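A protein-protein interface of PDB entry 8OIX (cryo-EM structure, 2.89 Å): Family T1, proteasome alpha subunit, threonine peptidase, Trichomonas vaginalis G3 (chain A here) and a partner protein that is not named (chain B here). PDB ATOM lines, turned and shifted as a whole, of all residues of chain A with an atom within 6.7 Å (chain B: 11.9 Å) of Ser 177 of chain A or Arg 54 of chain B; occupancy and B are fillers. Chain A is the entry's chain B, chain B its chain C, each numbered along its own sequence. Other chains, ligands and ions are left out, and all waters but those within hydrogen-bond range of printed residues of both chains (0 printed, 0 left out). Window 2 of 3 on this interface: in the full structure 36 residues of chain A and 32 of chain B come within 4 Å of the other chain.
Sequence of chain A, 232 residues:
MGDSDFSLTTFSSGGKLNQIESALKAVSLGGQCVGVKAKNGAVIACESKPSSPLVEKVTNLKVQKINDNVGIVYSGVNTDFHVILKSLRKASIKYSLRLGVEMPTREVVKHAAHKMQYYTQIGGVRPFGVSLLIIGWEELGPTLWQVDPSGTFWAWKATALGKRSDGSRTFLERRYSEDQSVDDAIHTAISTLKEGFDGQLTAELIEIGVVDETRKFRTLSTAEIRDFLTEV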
ATOM      1  N   VAL A  36      -7.613   4.388  14.699  1.00  0.00           N
ATOM      2  CA  VAL A  36      -8.946   4.183  14.142  1.00  0.00           C
ATOM      3  C   VAL A  36      -9.950   4.094  15.281  1.00  0.00           C
ATOM      4  O   VAL A  36      -9.798   3.265  16.183  1.00  0.00           O
ATOM      5  CB  VAL A  36      -9.009   2.910  13.273  1.00  0.00           C
ATOM      6  CG1 VAL A  36     -10.391   2.744  12.679  1.00  0.00           C
ATOM      7  CG2 VAL A  36      -7.964   2.957  12.172  1.00  0.00           C
ATOM      8  N   LYS A  37     -10.980   4.937  15.239  1.00  0.00           N
ATOM      9  CA  LYS A  37     -12.027   4.932  16.257  1.00  0.00           C
ATOM     10  C   LYS A  37     -13.202   4.093  15.766  1.00  0.00           C
ATOM     11  O   LYS A  37     -13.873   4.461  14.796  1.00  0.00           O
ATOM     12  CB  LYS A  37     -12.476   6.353  16.585  1.00  0.00           C
ATOM     13  CG  LYS A  37     -13.419   6.443  17.768  1.00  0.00           C
ATOM     14  CD  LYS A  37     -14.272   7.692  17.691  1.00  0.00           C
ATOM     15  CE  LYS A  37     -15.322   7.552  16.605  1.00  0.00           C
ATOM     16  NZ  LYS A  37     -16.146   8.779  16.450  1.00  0.00           N
ATOM     17  N   ALA A  38     -13.449   2.971  16.431  1.00  0.00           N
ATOM     18  CA  ALA A  38     -14.574   2.097  16.157  1.00  0.00           C
ATOM     19  C   ALA A  38     -15.775   2.530  16.997  1.00  0.00           C
ATOM     20  O   ALA A  38     -15.688   3.435  17.827  1.00  0.00           O
ATOM     21  CB  ALA A  38     -14.200   0.648  16.454  1.00  0.00           C
ATOM     22  N   LYS A  39     -16.917   1.879  16.764  1.00  0.00           N
ATOM     23  CA  LYS A  39     -18.097   2.157  17.578  1.00  0.00           C
ATOM     24  C   LYS A  39     -17.860   1.803  19.040  1.00  0.00           C
ATOM     25  O   LYS A  39     -18.110   2.617  19.937  1.00  0.00           O
ATOM     26  CB  LYS A  39     -19.309   1.392  17.042  1.00  0.00           C
ATOM     27  CG  LYS A  39     -19.753   1.798  15.655  1.00  0.00           C
ATOM     28  CD  LYS A  39     -20.105   3.276  15.590  1.00  0.00           C
ATOM     29  CE  LYS A  39     -21.233   3.627  16.546  1.00  0.00           C
ATOM     30  NZ  LYS A  39     -21.624   5.057  16.427  1.00  0.00           N
ATOM     31  N   TRP A 156     -10.029  12.661  16.213  1.00  0.00           N
ATOM     32  CA  TRP A 156     -10.161  11.953  14.951  1.00  0.00           C
ATOM     33  C   TRP A 156     -11.003  10.699  15.110  1.00  0.00           C
ATOM     34  O   TRP A 156     -11.005  10.059  16.165  1.00  0.00           O
ATOM     35  CB  TRP A 156      -8.790  11.532  14.405  1.00  0.00           C
ATOM     36  CG  TRP A 156      -7.953  12.620  13.822  1.00  0.00           C
ATOM     37  CD1 TRP A 156      -6.985  13.336  14.459  1.00  0.00           C
ATOM     38  CD2 TRP A 156      -7.979  13.095  12.471  1.00  0.00           C
ATOM     39  NE1 TRP A 156      -6.414  14.236  13.594  1.00  0.00           N
ATOM     40  CE2 TRP A 156      -7.009  14.109  12.366  1.00  0.00           C
ATOM     41  CE3 TRP A 156      -8.734  12.767  11.343  1.00  0.00           C
ATOM     42  CZ2 TRP A 156      -6.775  14.796  11.180  1.00  0.00           C
ATOM     43  CZ3 TRP A 156      -8.498  13.450  10.165  1.00  0.00           C
ATOM     44  CH2 TRP A 156      -7.528  14.454  10.094  1.00  0.00           C
ATOM     45  N   LYS A 157     -11.730  10.359  14.045  1.00  0.00           N
ATOM     46  CA  LYS A 157     -12.286   9.018  13.919  1.00  0.00           C
ATOM     47  C   LYS A 157     -11.228   8.043  13.422  1.00  0.00           C
ATOM     48  O   LYS A 157     -11.259   6.861  13.779  1.00  0.00           O
ATOM     49  CB  LYS A 157     -13.497   9.027  12.985  1.00  0.00           C
ATOM     50  CG  LYS A 157     -14.661   9.852  13.503  1.00  0.00           C
ATOM     51  CD  LYS A 157     -15.919   9.613  12.692  1.00  0.00           C
ATOM     52  CE  LYS A 157     -15.849  10.332  11.356  1.00  0.00           C
ATOM     53  NZ  LYS A 157     -16.088  11.794  11.497  1.00  0.00           N
ATOM     54  N   LEU A 172      -7.317   6.017   4.757  1.00  0.00           N
ATOM     55  CA  LEU A 172      -8.336   5.975   5.802  1.00  0.00           C
ATOM     56  C   LEU A 172      -9.609   6.692   5.367  1.00  0.00           C
ATOM     57  O   LEU A 172     -10.713   6.188   5.590  1.00  0.00           O
ATOM     58  CB  LEU A 172      -7.785   6.576   7.093  1.00  0.00           C
ATOM     59  CG  LEU A 172      -6.813   5.661   7.832  1.00  0.00           C
ATOM     60  CD1 LEU A 172      -6.095   6.420   8.916  1.00  0.00           C
ATOM     61  CD2 LEU A 172      -7.565   4.484   8.423  1.00  0.00           C
ATOM     62  N   GLU A 173      -9.474   7.862   4.739  1.00  0.00           N
ATOM     63  CA  GLU A 173     -10.637   8.565   4.205  1.00  0.00           C
ATOM     64  C   GLU A 173     -11.421   7.676   3.252  1.00  0.00           C
ATOM     65  O   GLU A 173     -12.654   7.743   3.194  1.00  0.00           O
ATOM     66  CB  GLU A 173     -10.190   9.844   3.495  1.00  0.00           C
ATOM     67  CG  GLU A 173      -9.912  11.019   4.416  1.00  0.00           C
ATOM     68  CD  GLU A 173     -11.090  11.967   4.522  1.00  0.00           C
ATOM     69  OE1 GLU A 173     -11.982  11.903   3.650  1.00  0.00           O
ATOM     70  OE2 GLU A 173     -11.124  12.775   5.472  1.00  0.00           O
ATOM     71  N   ARG A 174     -10.719   6.832   2.501  1.00  0.00           N
ATOM     72  CA  ARG A 174     -11.348   5.989   1.496  1.00  0.00           C
ATOM     73  C   ARG A 174     -11.908   4.690   2.062  1.00  0.00           C
ATOM     74  O   ARG A 174     -12.912   4.186   1.547  1.00  0.00           O
ATOM     75  CB  ARG A 174     -10.327   5.674   0.399  1.00  0.00           C
ATOM     76  CG  ARG A 174     -10.820   4.813  -0.744  1.00  0.00           C
ATOM     77  CD  ARG A 174      -9.657   4.454  -1.656  1.00  0.00           C
ATOM     78  NE  ARG A 174      -8.946   5.641  -2.114  1.00  0.00           N
ATOM     79  CZ  ARG A 174      -7.688   5.928  -1.808  1.00  0.00           C
ATOM     80  NH1 ARG A 174      -6.950   5.110  -1.075  1.00  0.00           N
ATOM     81  NH2 ARG A 174      -7.153   7.062  -2.254  1.00  0.00           N
ATOM     82  N   ARG A 175     -11.299   4.139   3.114  1.00  0.00           N
ATOM     83  CA  ARG A 175     -11.657   2.817   3.618  1.00  0.00           C
ATOM     84  C   ARG A 175     -12.028   2.825   5.101  1.00  0.00           C
ATOM     85  O   ARG A 175     -11.755   1.856   5.811  1.00  0.00           O
ATOM     86  CB  ARG A 175     -10.526   1.821   3.368  1.00  0.00           C
ATOM     87  CG  ARG A 175     -11.008   0.474   2.851  1.00  0.00           C
ATOM     88  CD  ARG A 175     -10.057  -0.651   3.219  1.00  0.00           C
ATOM     89  NE  ARG A 175     -10.154  -1.006   4.630  1.00  0.00           N
ATOM     90  CZ  ARG A 175      -9.503  -2.014   5.195  1.00  0.00           C
ATOM     91  NH1 ARG A 175      -8.613  -2.724   4.522  1.00  0.00           N
ATOM     92  NH2 ARG A 175      -9.728  -2.297   6.475  1.00  0.00           N
ATOM     93  N   TYR A 176     -12.642   3.898   5.591  1.00  0.00           N
ATOM     94  CA  TYR A 176     -13.099   3.953   6.974  1.00  0.00           C
ATOM     95  C   TYR A 176     -14.612   4.096   7.013  1.00  0.00           C
ATOM     96  O   TYR A 176     -15.205   4.799   6.191  1.00  0.00           O
ATOM     97  CB  TYR A 176     -12.448   5.107   7.749  1.00  0.00           C
ATOM     98  CG  TYR A 176     -12.984   5.304   9.151  1.00  0.00           C
ATOM     99  CD1 TYR A 176     -12.456   4.600  10.222  1.00  0.00           C
ATOM    100  CD2 TYR A 176     -14.005   6.211   9.404  1.00  0.00           C
ATOM    101  CE1 TYR A 176     -12.942   4.780  11.503  1.00  0.00           C
ATOM    102  CE2 TYR A 176     -14.495   6.398  10.683  1.00  0.00           C
ATOM    103  CZ  TYR A 176     -13.958   5.680  11.727  1.00  0.00           C
ATOM    104  OH  TYR A 176     -14.441   5.861  13.001  1.00  0.00           O
ATOM    105  N   SER A 177     -15.226   3.420   7.980  1.00  0.00           N
ATOM    106  CA  SER A 177     -16.643   3.561   8.274  1.00  0.00           C
ATOM    107  C   SER A 177     -16.821   3.552   9.782  1.00  0.00           C
ATOM    108  O   SER A 177     -16.087   2.862  10.495  1.00  0.00           O
ATOM    109  CB  SER A 177     -17.468   2.439   7.630  1.00  0.00           C
ATOM    110  OG  SER A 177     -16.980   1.163   8.007  1.00  0.00           O
ATOM    111  N   GLU A 178     -17.782   4.341  10.266  1.00  0.00           N
ATOM    112  CA  GLU A 178     -18.001   4.430  11.706  1.00  0.00           C
ATOM    113  C   GLU A 178     -18.391   3.081  12.295  1.00  0.00           C
ATOM    114  O   GLU A 178     -17.884   2.687  13.351  1.00  0.00           O
ATOM    115  CB  GLU A 178     -19.078   5.472  12.011  1.00  0.00           C
ATOM    116  CG  GLU A 178     -18.568   6.899  12.108  1.00  0.00           C
ATOM    117  CD  GLU A 178     -18.570   7.613  10.770  1.00  0.00           C
ATOM    118  OE1 GLU A 178     -18.546   6.929   9.726  1.00  0.00           O
ATOM    119  OE2 GLU A 178     -18.607   8.860  10.763  1.00  0.00           O
ATOM    120  N   ASP A 179     -19.264   2.345  11.605  1.00  0.00           N
ATOM    121  CA  ASP A 179     -19.864   1.120  12.126  1.00  0.00           C
ATOM    122  C   ASP A 179     -18.847   0.011  12.391  1.00  0.00           C
ATOM    123  O   ASP A 179     -19.218  -1.074  12.851  1.00  0.00           O
ATOM    124  CB  ASP A 179     -20.940   0.623  11.154  1.00  0.00           C
ATOM    125  CG  ASP A 179     -21.947  -0.301  11.814  1.00  0.00           C
ATOM    126  OD1 ASP A 179     -21.864  -0.500  13.045  1.00  0.00           O
ATOM    127  OD2 ASP A 179     -22.824  -0.831  11.100  1.00  0.00           O
ATOM    128  N   GLN A 180     -17.571   0.258  12.102  1.00  0.00           N
ATOM    129  CA  GLN A 180     -16.544  -0.749  12.341  1.00  0.00           C
ATOM    130  C   GLN A 180     -16.457  -1.093  13.823  1.00  0.00           C
ATOM    131  O   GLN A 180     -16.580  -0.224  14.688  1.00  0.00           O
ATOM    132  CB  GLN A 180     -15.185  -0.259  11.842  1.00  0.00           C
ATOM    133  CG  GLN A 180     -15.081  -0.106  10.338  1.00  0.00           C
ATOM    134  CD  GLN A 180     -13.745   0.465   9.907  1.00  0.00           C
ATOM    135  OE1 GLN A 180     -13.163   0.033   8.912  1.00  0.00           O
ATOM    136  NE2 GLN A 180     -13.250   1.441  10.658  1.00  0.00           N
ATOM    137  N   SER A 181     -16.272  -2.380  14.112  1.00  0.00           N
ATOM    138  CA  SER A 181     -16.032  -2.839  15.471  1.00  0.00           C
ATOM    139  C   SER A 181     -14.550  -2.702  15.815  1.00  0.00           C
ATOM    140  O   SER A 181     -13.739  -2.226  15.016  1.00  0.00           O
ATOM    141  CB  SER A 181     -16.503  -4.280  15.636  1.00  0.00           C
ATOM    142  OG  SER A 181     -15.770  -5.152  14.794  1.00  0.00           O
ATOM    143  N   THR A 188      -8.439  -2.333   9.999  1.00  0.00           N
ATOM    144  CA  THR A 188      -8.243  -1.099   9.244  1.00  0.00           C
ATOM    145  C   THR A 188      -6.881  -0.484   9.537  1.00  0.00           C
ATOM    146  O   THR A 188      -6.187  -0.031   8.621  1.00  0.00           O
ATOM    147  CB  THR A 188      -9.359  -0.105   9.567  1.00  0.00           C
ATOM    148  OG1 THR A 188     -10.622  -0.666   9.193  1.00  0.00           O
ATOM    149  CG2 THR A 188      -9.149   1.197   8.812  1.00  0.00           C
ATOM    150  N   LYS B  49     -13.964  25.595  13.022  1.00  0.00           N
ATOM    151  CA  LYS B  49     -12.983  24.656  13.542  1.00  0.00           C
ATOM    152  C   LYS B  49     -11.762  24.606  12.633  1.00  0.00           C
ATOM    153  O   LYS B  49     -11.874  24.641  11.405  1.00  0.00           O
ATOM    154  CB  LYS B  49     -13.588  23.259  13.675  1.00  0.00           C
ATOM    155  CG  LYS B  49     -14.705  23.133  14.689  1.00  0.00           C
ATOM    156  CD  LYS B  49     -15.241  21.713  14.695  1.00  0.00           C
ATOM    157  CE  LYS B  49     -16.464  21.556  15.580  1.00  0.00           C
ATOM    158  NZ  LYS B  49     -16.103  21.506  17.023  1.00  0.00           N
ATOM    159  N   LYS B  50     -10.585  24.527  13.250  1.00  0.00           N
ATOM    160  CA  LYS B  50      -9.354  24.391  12.484  1.00  0.00           C
ATOM    161  C   LYS B  50      -9.200  22.986  11.927  1.00  0.00           C
ATOM    162  O   LYS B  50      -8.616  22.807  10.851  1.00  0.00           O
ATOM    163  CB  LYS B  50      -8.149  24.746  13.358  1.00  0.00           C
ATOM    164  CG  LYS B  50      -6.814  24.725  12.638  1.00  0.00           C
ATOM    165  CD  LYS B  50      -5.681  25.072  13.591  1.00  0.00           C
ATOM    166  CE  LYS B  50      -4.327  24.783  12.969  1.00  0.00           C
ATOM    167  NZ  LYS B  50      -4.118  23.323  12.773  1.00  0.00           N
ATOM    168  N   ASN B  51      -9.723  21.989  12.630  1.00  0.00           N
ATOM    169  CA  ASN B  51      -9.590  20.588  12.247  1.00  0.00           C
ATOM    170  C   ASN B  51     -10.944  20.145  11.706  1.00  0.00           C
ATOM    171  O   ASN B  51     -11.858  19.839  12.476  1.00  0.00           O
ATOM    172  CB  ASN B  51      -9.164  19.758  13.450  1.00  0.00           C
ATOM    173  CG  ASN B  51      -8.113  20.458  14.286  1.00  0.00           C
ATOM    174  OD1 ASN B  51      -8.269  20.611  15.496  1.00  0.00           O
ATOM    175  ND2 ASN B  51      -7.080  20.965  13.631  1.00  0.00           N
ATOM    176  N   THR B  52     -11.075  20.112  10.381  1.00  0.00           N
ATOM    177  CA  THR B  52     -12.352  19.827   9.728  1.00  0.00           C
ATOM    178  C   THR B  52     -12.134  18.839   8.586  1.00  0.00           C
ATOM    179  O   THR B  52     -11.741  19.232   7.483  1.00  0.00           O
ATOM    180  CB  THR B  52     -12.994  21.113   9.221  1.00  0.00           C
ATOM    181  OG1 THR B  52     -12.012  21.899   8.536  1.00  0.00           O
ATOM    182  CG2 THR B  52     -13.540  21.917  10.383  1.00  0.00           C
ATOM    183  N   GLY B  53     -12.394  17.558   8.851  1.00  0.00           N
ATOM    184  CA  GLY B  53     -12.261  16.533   7.840  1.00  0.00           C
ATOM    185  C   GLY B  53     -13.396  15.535   7.934  1.00  0.00           C
ATOM    186  O   GLY B  53     -14.184  15.548   8.883  1.00  0.00           O
ATOM    187  N   ARG B  54     -13.472  14.666   6.923  1.00  0.00           N
ATOM    188  CA  ARG B  54     -14.437  13.574   6.965  1.00  0.00           C
ATOM    189  C   ARG B  54     -14.111  12.607   8.096  1.00  0.00           C
ATOM    190  O   ARG B  54     -15.012  11.941   8.615  1.00  0.00           O
ATOM    191  CB  ARG B  54     -14.461  12.865   5.602  1.00  0.00           C
ATOM    192  CG  ARG B  54     -14.468  11.333   5.600  1.00  0.00           C
ATOM    193  CD  ARG B  54     -15.829  10.747   5.964  1.00  0.00           C
ATOM    194  NE  ARG B  54     -15.706   9.435   6.587  1.00  0.00           N
ATOM    195  CZ  ARG B  54     -16.724   8.727   7.055  1.00  0.00           C
ATOM    196  NH1 ARG B  54     -17.916   9.270   7.239  1.00  0.00           N
ATOM    197  NH2 ARG B  54     -16.520   7.466   7.426  1.00  0.00           N
ATOM    198  N   LEU B  55     -12.854  12.574   8.530  1.00  0.00           N
ATOM    199  CA  LEU B  55     -12.406  11.701   9.604  1.00  0.00           C
ATOM    200  C   LEU B  55     -12.373  12.397  10.956  1.00  0.00           C
ATOM    201  O   LEU B  55     -12.473  11.723  11.984  1.00  0.00           O
ATOM    202  CB  LEU B  55     -11.019  11.137   9.283  1.00  0.00           C
ATOM    203  CG  LEU B  55     -10.965  10.202   8.075  1.00  0.00           C
ATOM    204  CD1 LEU B  55      -9.551   9.708   7.837  1.00  0.00           C
ATOM    205  CD2 LEU B  55     -11.914   9.033   8.269  1.00  0.00           C
ATOM    206  N   VAL B  56     -12.198  13.720  10.982  1.00  0.00           N
ATOM    207  CA  VAL B  56     -12.094  14.432  12.251  1.00  0.00           C
ATOM    208  C   VAL B  56     -13.378  14.242  13.043  1.00  0.00           C
ATOM    209  O   VAL B  56     -14.480  14.517  12.552  1.00  0.00           O
ATOM    210  CB  VAL B  56     -11.803  15.919  12.008  1.00  0.00           C
ATOM    211  CG1 VAL B  56     -11.955  16.705  13.298  1.00  0.00           C
ATOM    212  CG2 VAL B  56     -10.413  16.102  11.434  1.00  0.00           C
ATOM    213  N   ASP B  57     -13.240  13.766  14.275  1.00  0.00           N
ATOM    214  CA  ASP B  57     -14.376  13.529  15.158  1.00  0.00           C
ATOM    215  C   ASP B  57     -14.631  14.793  15.970  1.00  0.00           C
ATOM    216  O   ASP B  57     -13.858  15.127  16.871  1.00  0.00           O
ATOM    217  CB  ASP B  57     -14.105  12.329  16.061  1.00  0.00           C
ATOM    218  CG  ASP B  57     -15.367  11.767  16.674  1.00  0.00           C
ATOM    219  OD1 ASP B  57     -16.468  12.198  16.277  1.00  0.00           O
ATOM    220  OD2 ASP B  57     -15.254  10.874  17.539  1.00  0.00           O
ATOM    221  N   TYR B  58     -15.717  15.498  15.654  1.00  0.00           N
ATOM    222  CA  TYR B  58     -16.039  16.766  16.308  1.00  0.00           C
ATOM    223  C   TYR B  58     -16.617  16.524  17.706  1.00  0.00           C
ATOM    224  O   TYR B  58     -17.742  16.898  18.032  1.00  0.00           O
ATOM    225  CB  TYR B  58     -16.994  17.563  15.431  1.00  0.00           C
ATOM    226  CG  TYR B  58     -16.537  17.647  13.994  1.00  0.00           C
ATOM    227  CD1 TYR B  58     -15.533  18.523  13.615  1.00  0.00           C
ATOM    228  CD2 TYR B  58     -17.104  16.840  13.019  1.00  0.00           C
ATOM    229  CE1 TYR B  58     -15.107  18.601  12.305  1.00  0.00           C
ATOM    230  CE2 TYR B  58     -16.685  16.911  11.703  1.00  0.00           C
ATOM    231  CZ  TYR B  58     -15.687  17.794  11.352  1.00  0.00           C
ATOM    232  OH  TYR B  58     -15.264  17.870  10.046  1.00  0.00           O
ATOM    233  N   LEU B  59     -15.802  15.873  18.538  1.00  0.00           N
ATOM    234  CA  LEU B  59     -16.252  15.443  19.860  1.00  0.00           C
ATOM    235  C   LEU B  59     -16.527  16.628  20.777  1.00  0.00           C
ATOM    236  O   LEU B  59     -17.596  16.714  21.393  1.00  0.00           O
ATOM    237  CB  LEU B  59     -15.205  14.522  20.477  1.00  0.00           C
ATOM    238  CG  LEU B  59     -15.130  13.142  19.837  1.00  0.00           C
ATOM    239  CD1 LEU B  59     -13.984  12.360  20.425  1.00  0.00           C
ATOM    240  CD2 LEU B  59     -16.444  12.413  20.052  1.00  0.00           C
ATOM    241  N   SER B 203     -17.379  23.266   1.908  1.00  0.00           N
ATOM    242  CA  SER B 203     -17.369  24.365   2.865  1.00  0.00           C
ATOM    243  C   SER B 203     -18.738  24.538   3.514  1.00  0.00           C
ATOM    244  O   SER B 203     -19.709  23.894   3.115  1.00  0.00           O
ATOM    245  CB  SER B 203     -16.941  25.666   2.182  1.00  0.00           C
ATOM    246  OG  SER B 203     -16.829  26.724   3.119  1.00  0.00           O
ATOM    247  N   SER B 205     -20.025  23.498   6.079  1.00  0.00           N
ATOM    248  CA  SER B 205     -20.606  22.363   6.783  1.00  0.00           C
ATOM    249  C   SER B 205     -20.862  22.710   8.245  1.00  0.00           C
ATOM    250  O   SER B 205     -20.038  23.352   8.901  1.00  0.00           O
ATOM    251  CB  SER B 205     -19.683  21.150   6.677  1.00  0.00           C
ATOM    252  OG  SER B 205     -20.283  20.001   7.251  1.00  0.00           O
ATOM    253  N   ALA B 206     -22.026  22.290   8.749  1.00  0.00           N
ATOM    254  CA  ALA B 206     -22.412  22.617  10.119  1.00  0.00           C
ATOM    255  C   ALA B 206     -21.399  22.094  11.128  1.00  0.00           C
ATOM    256  O   ALA B 206     -21.023  22.807  12.066  1.00  0.00           O
ATOM    257  CB  ALA B 206     -23.800  22.057  10.422  1.00  0.00           C
ATOM    258  N   ASP B 207     -20.948  20.848  10.959  1.00  0.00           N
ATOM    259  CA  ASP B 207     -19.995  20.273  11.900  1.00  0.00           C
ATOM    260  C   ASP B 207     -18.661  21.005  11.889  1.00  0.00           C
ATOM    261  O   ASP B 207     -17.867  20.838  12.820  1.00  0.00           O
ATOM    262  CB  ASP B 207     -19.790  18.785  11.603  1.00  0.00           C
ATOM    263  CG  ASP B 207     -19.506  18.515  10.140  1.00  0.00           C
ATOM    264  OD1 ASP B 207     -19.562  19.469   9.339  1.00  0.00           O
ATOM    265  OD2 ASP B 207     -19.229  17.349   9.793  1.00  0.00           O
ATOM    266  N   LYS B 208     -18.395  21.808  10.858  1.00  0.00           N
ATOM    267  CA  LYS B 208     -17.197  22.634  10.816  1.00  0.00           C
ATOM    268  C   LYS B 208     -17.327  23.898  11.657  1.00  0.00           C
ATOM    269  O   LYS B 208     -16.324  24.586  11.870  1.00  0.00           O
ATOM    270  CB  LYS B 208     -16.877  23.025   9.371  1.00  0.00           C
ATOM    271  CG  LYS B 208     -16.520  21.859   8.465  1.00  0.00           C
ATOM    272  CD  LYS B 208     -16.171  22.347   7.068  1.00  0.00           C
ATOM    273  CE  LYS B 208     -15.007  23.326   7.097  1.00  0.00           C
ATOM    274  NZ  LYS B 208     -14.591  23.742   5.730  1.00  0.00           N
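O of Lys 157 of chain A is in hydrogen-bond range of N of Lys 37 of chain A (2.4 Å). The side-chain hydroxyl of Tyr 176 of chain A sits close to the backbone carbonyl oxygen of Lys 157 of chain A, 3.4 Å away. The side-chain amino group of Lys 157 of chain A lies within salt-bridge range of the side-chain carboxylate of Glu 178 of chain A, 3.9 Å away. The backbone carbonyl oxygen of Ser 177 of chain A sits close to the side-chain amide nitrogen of Gln 180 of chain A (3.2 Å).
Printed residues of chain B within 4 Å of Lys 37 of chain A: Asp 57. No residue of chain B comes within 4 Å of Ala 38 of chain A. Of the printed residues of chain B, Leu 172 of chain A touches Leu 55 (3.7 Å). Of chain B, only Arg 54 (3.2 Å) and Leu 55 (3.5 Å) come within 4 Å of Glu 173 of chain A. Of the printed residues of chain B, Tyr 176 of chain A touches Arg 54 (3.2 Å) and Leu 55 (3.7 Å). Printed residues of chain B within 4 Å of Ser 177 of chain A: Arg 54 (3.998 Å). Glu 178 of chain A touches just one residue of chain B: Arg 54 (3.1 Å). No residue of chain B comes within 4 Å of Asp 179 of chain A. No residue of chain B comes within 4 Å of Gln 180 of chain A. Asn 51 of chain B touches none of the printed residues of chain A. Printed residues of chain A within 4 Å of Arg 54 of chain B: Lys 157, Glu 173, Tyr 176, Ser 177 and Glu 178. Printed residues of chain A within 4 Å of Asp 57 of chain B: Lys 37 (2.5 Å), Trp 156 (3.6 Å) and Lys 157 (3.6 Å). Ala 206 of chain B touches none of the printed residues of chain A. The nearest printed residue of chain A that does not touch Arg 54 of chain B is Leu 172 of chain A (6.0 Å). The nearest printed residue of chain B that does not touch Leu 172 of chain A is Arg 54 of chain B (6.0 Å).
Among the printed residues, merely in contact across the chains: Trp 156 of chain A with Leu 55 of chain B, Trp 156 of chain A with Val 56 of chain B, Trp 156 of chain A with Asp 57 of chain B, Lys 157 of chain A with Asp 57 of chain B, Leu 172 of chain A with Leu 55 of chain B, Glu 173 of chain A with Leu 55 of chain B, Tyr 176 of chain A with Leu 55 of chain B and Ser 177 of chain A with Arg 54 of chain B.
Of the 16 printed residues of chain B, 4 touch a printed residue of chain A. Hydrophobic or aromatic side chains of chain B within 4 Å of the printed part of chain A: Leu 55 and Val 56. Of the 17 printed residues of chain A, 8 touch a printed residue of chain B. Among the printed residues, Asp or Glu carboxylates within 4 Å of a Lys or Arg side-chain nitrogen of the other chain: Lys 37 of chain A with Asp 57 of chain B (2.5 Å) and Glu 178 of chain A with Arg 54 of chain B (3.1 Å).
NZ of Lys 37 of chain A is in salt-bridge range of OD2 of Asp 57 of chain B (2.5 Å). The backbone carbonyl oxygen of Arg 54 of chain B sits at hydrogen-bond distance from the side-chain amino group of Lys 157 of chain A (3.1 Å). The backbone carbonyl oxygen of Leu 55 of chain B sits at hydrogen-bond distance from the backbone NH of Lys 157 of chain A (2.6 Å). NZ of Lys 157 of chain A sits at hydrogen-bond distance from O of Val 56 of chain B, 3.3 Å away. The backbone NH (N) of Arg 54 of chain B sits close to the side-chain carboxylate (OE2) of Glu 173 of chain A, 3.3 Å away. The backbone carbonyl oxygen of Tyr 176 of chain A sits at hydrogen-bond distance from the guanidinium group of Arg 54 of chain B (3.2 Å). The guanidinium group (NH2) of Arg 54 of chain B is in salt-bridge range of the side-chain carboxylate (OE1) of Glu 178 of chain A (3.1 Å).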
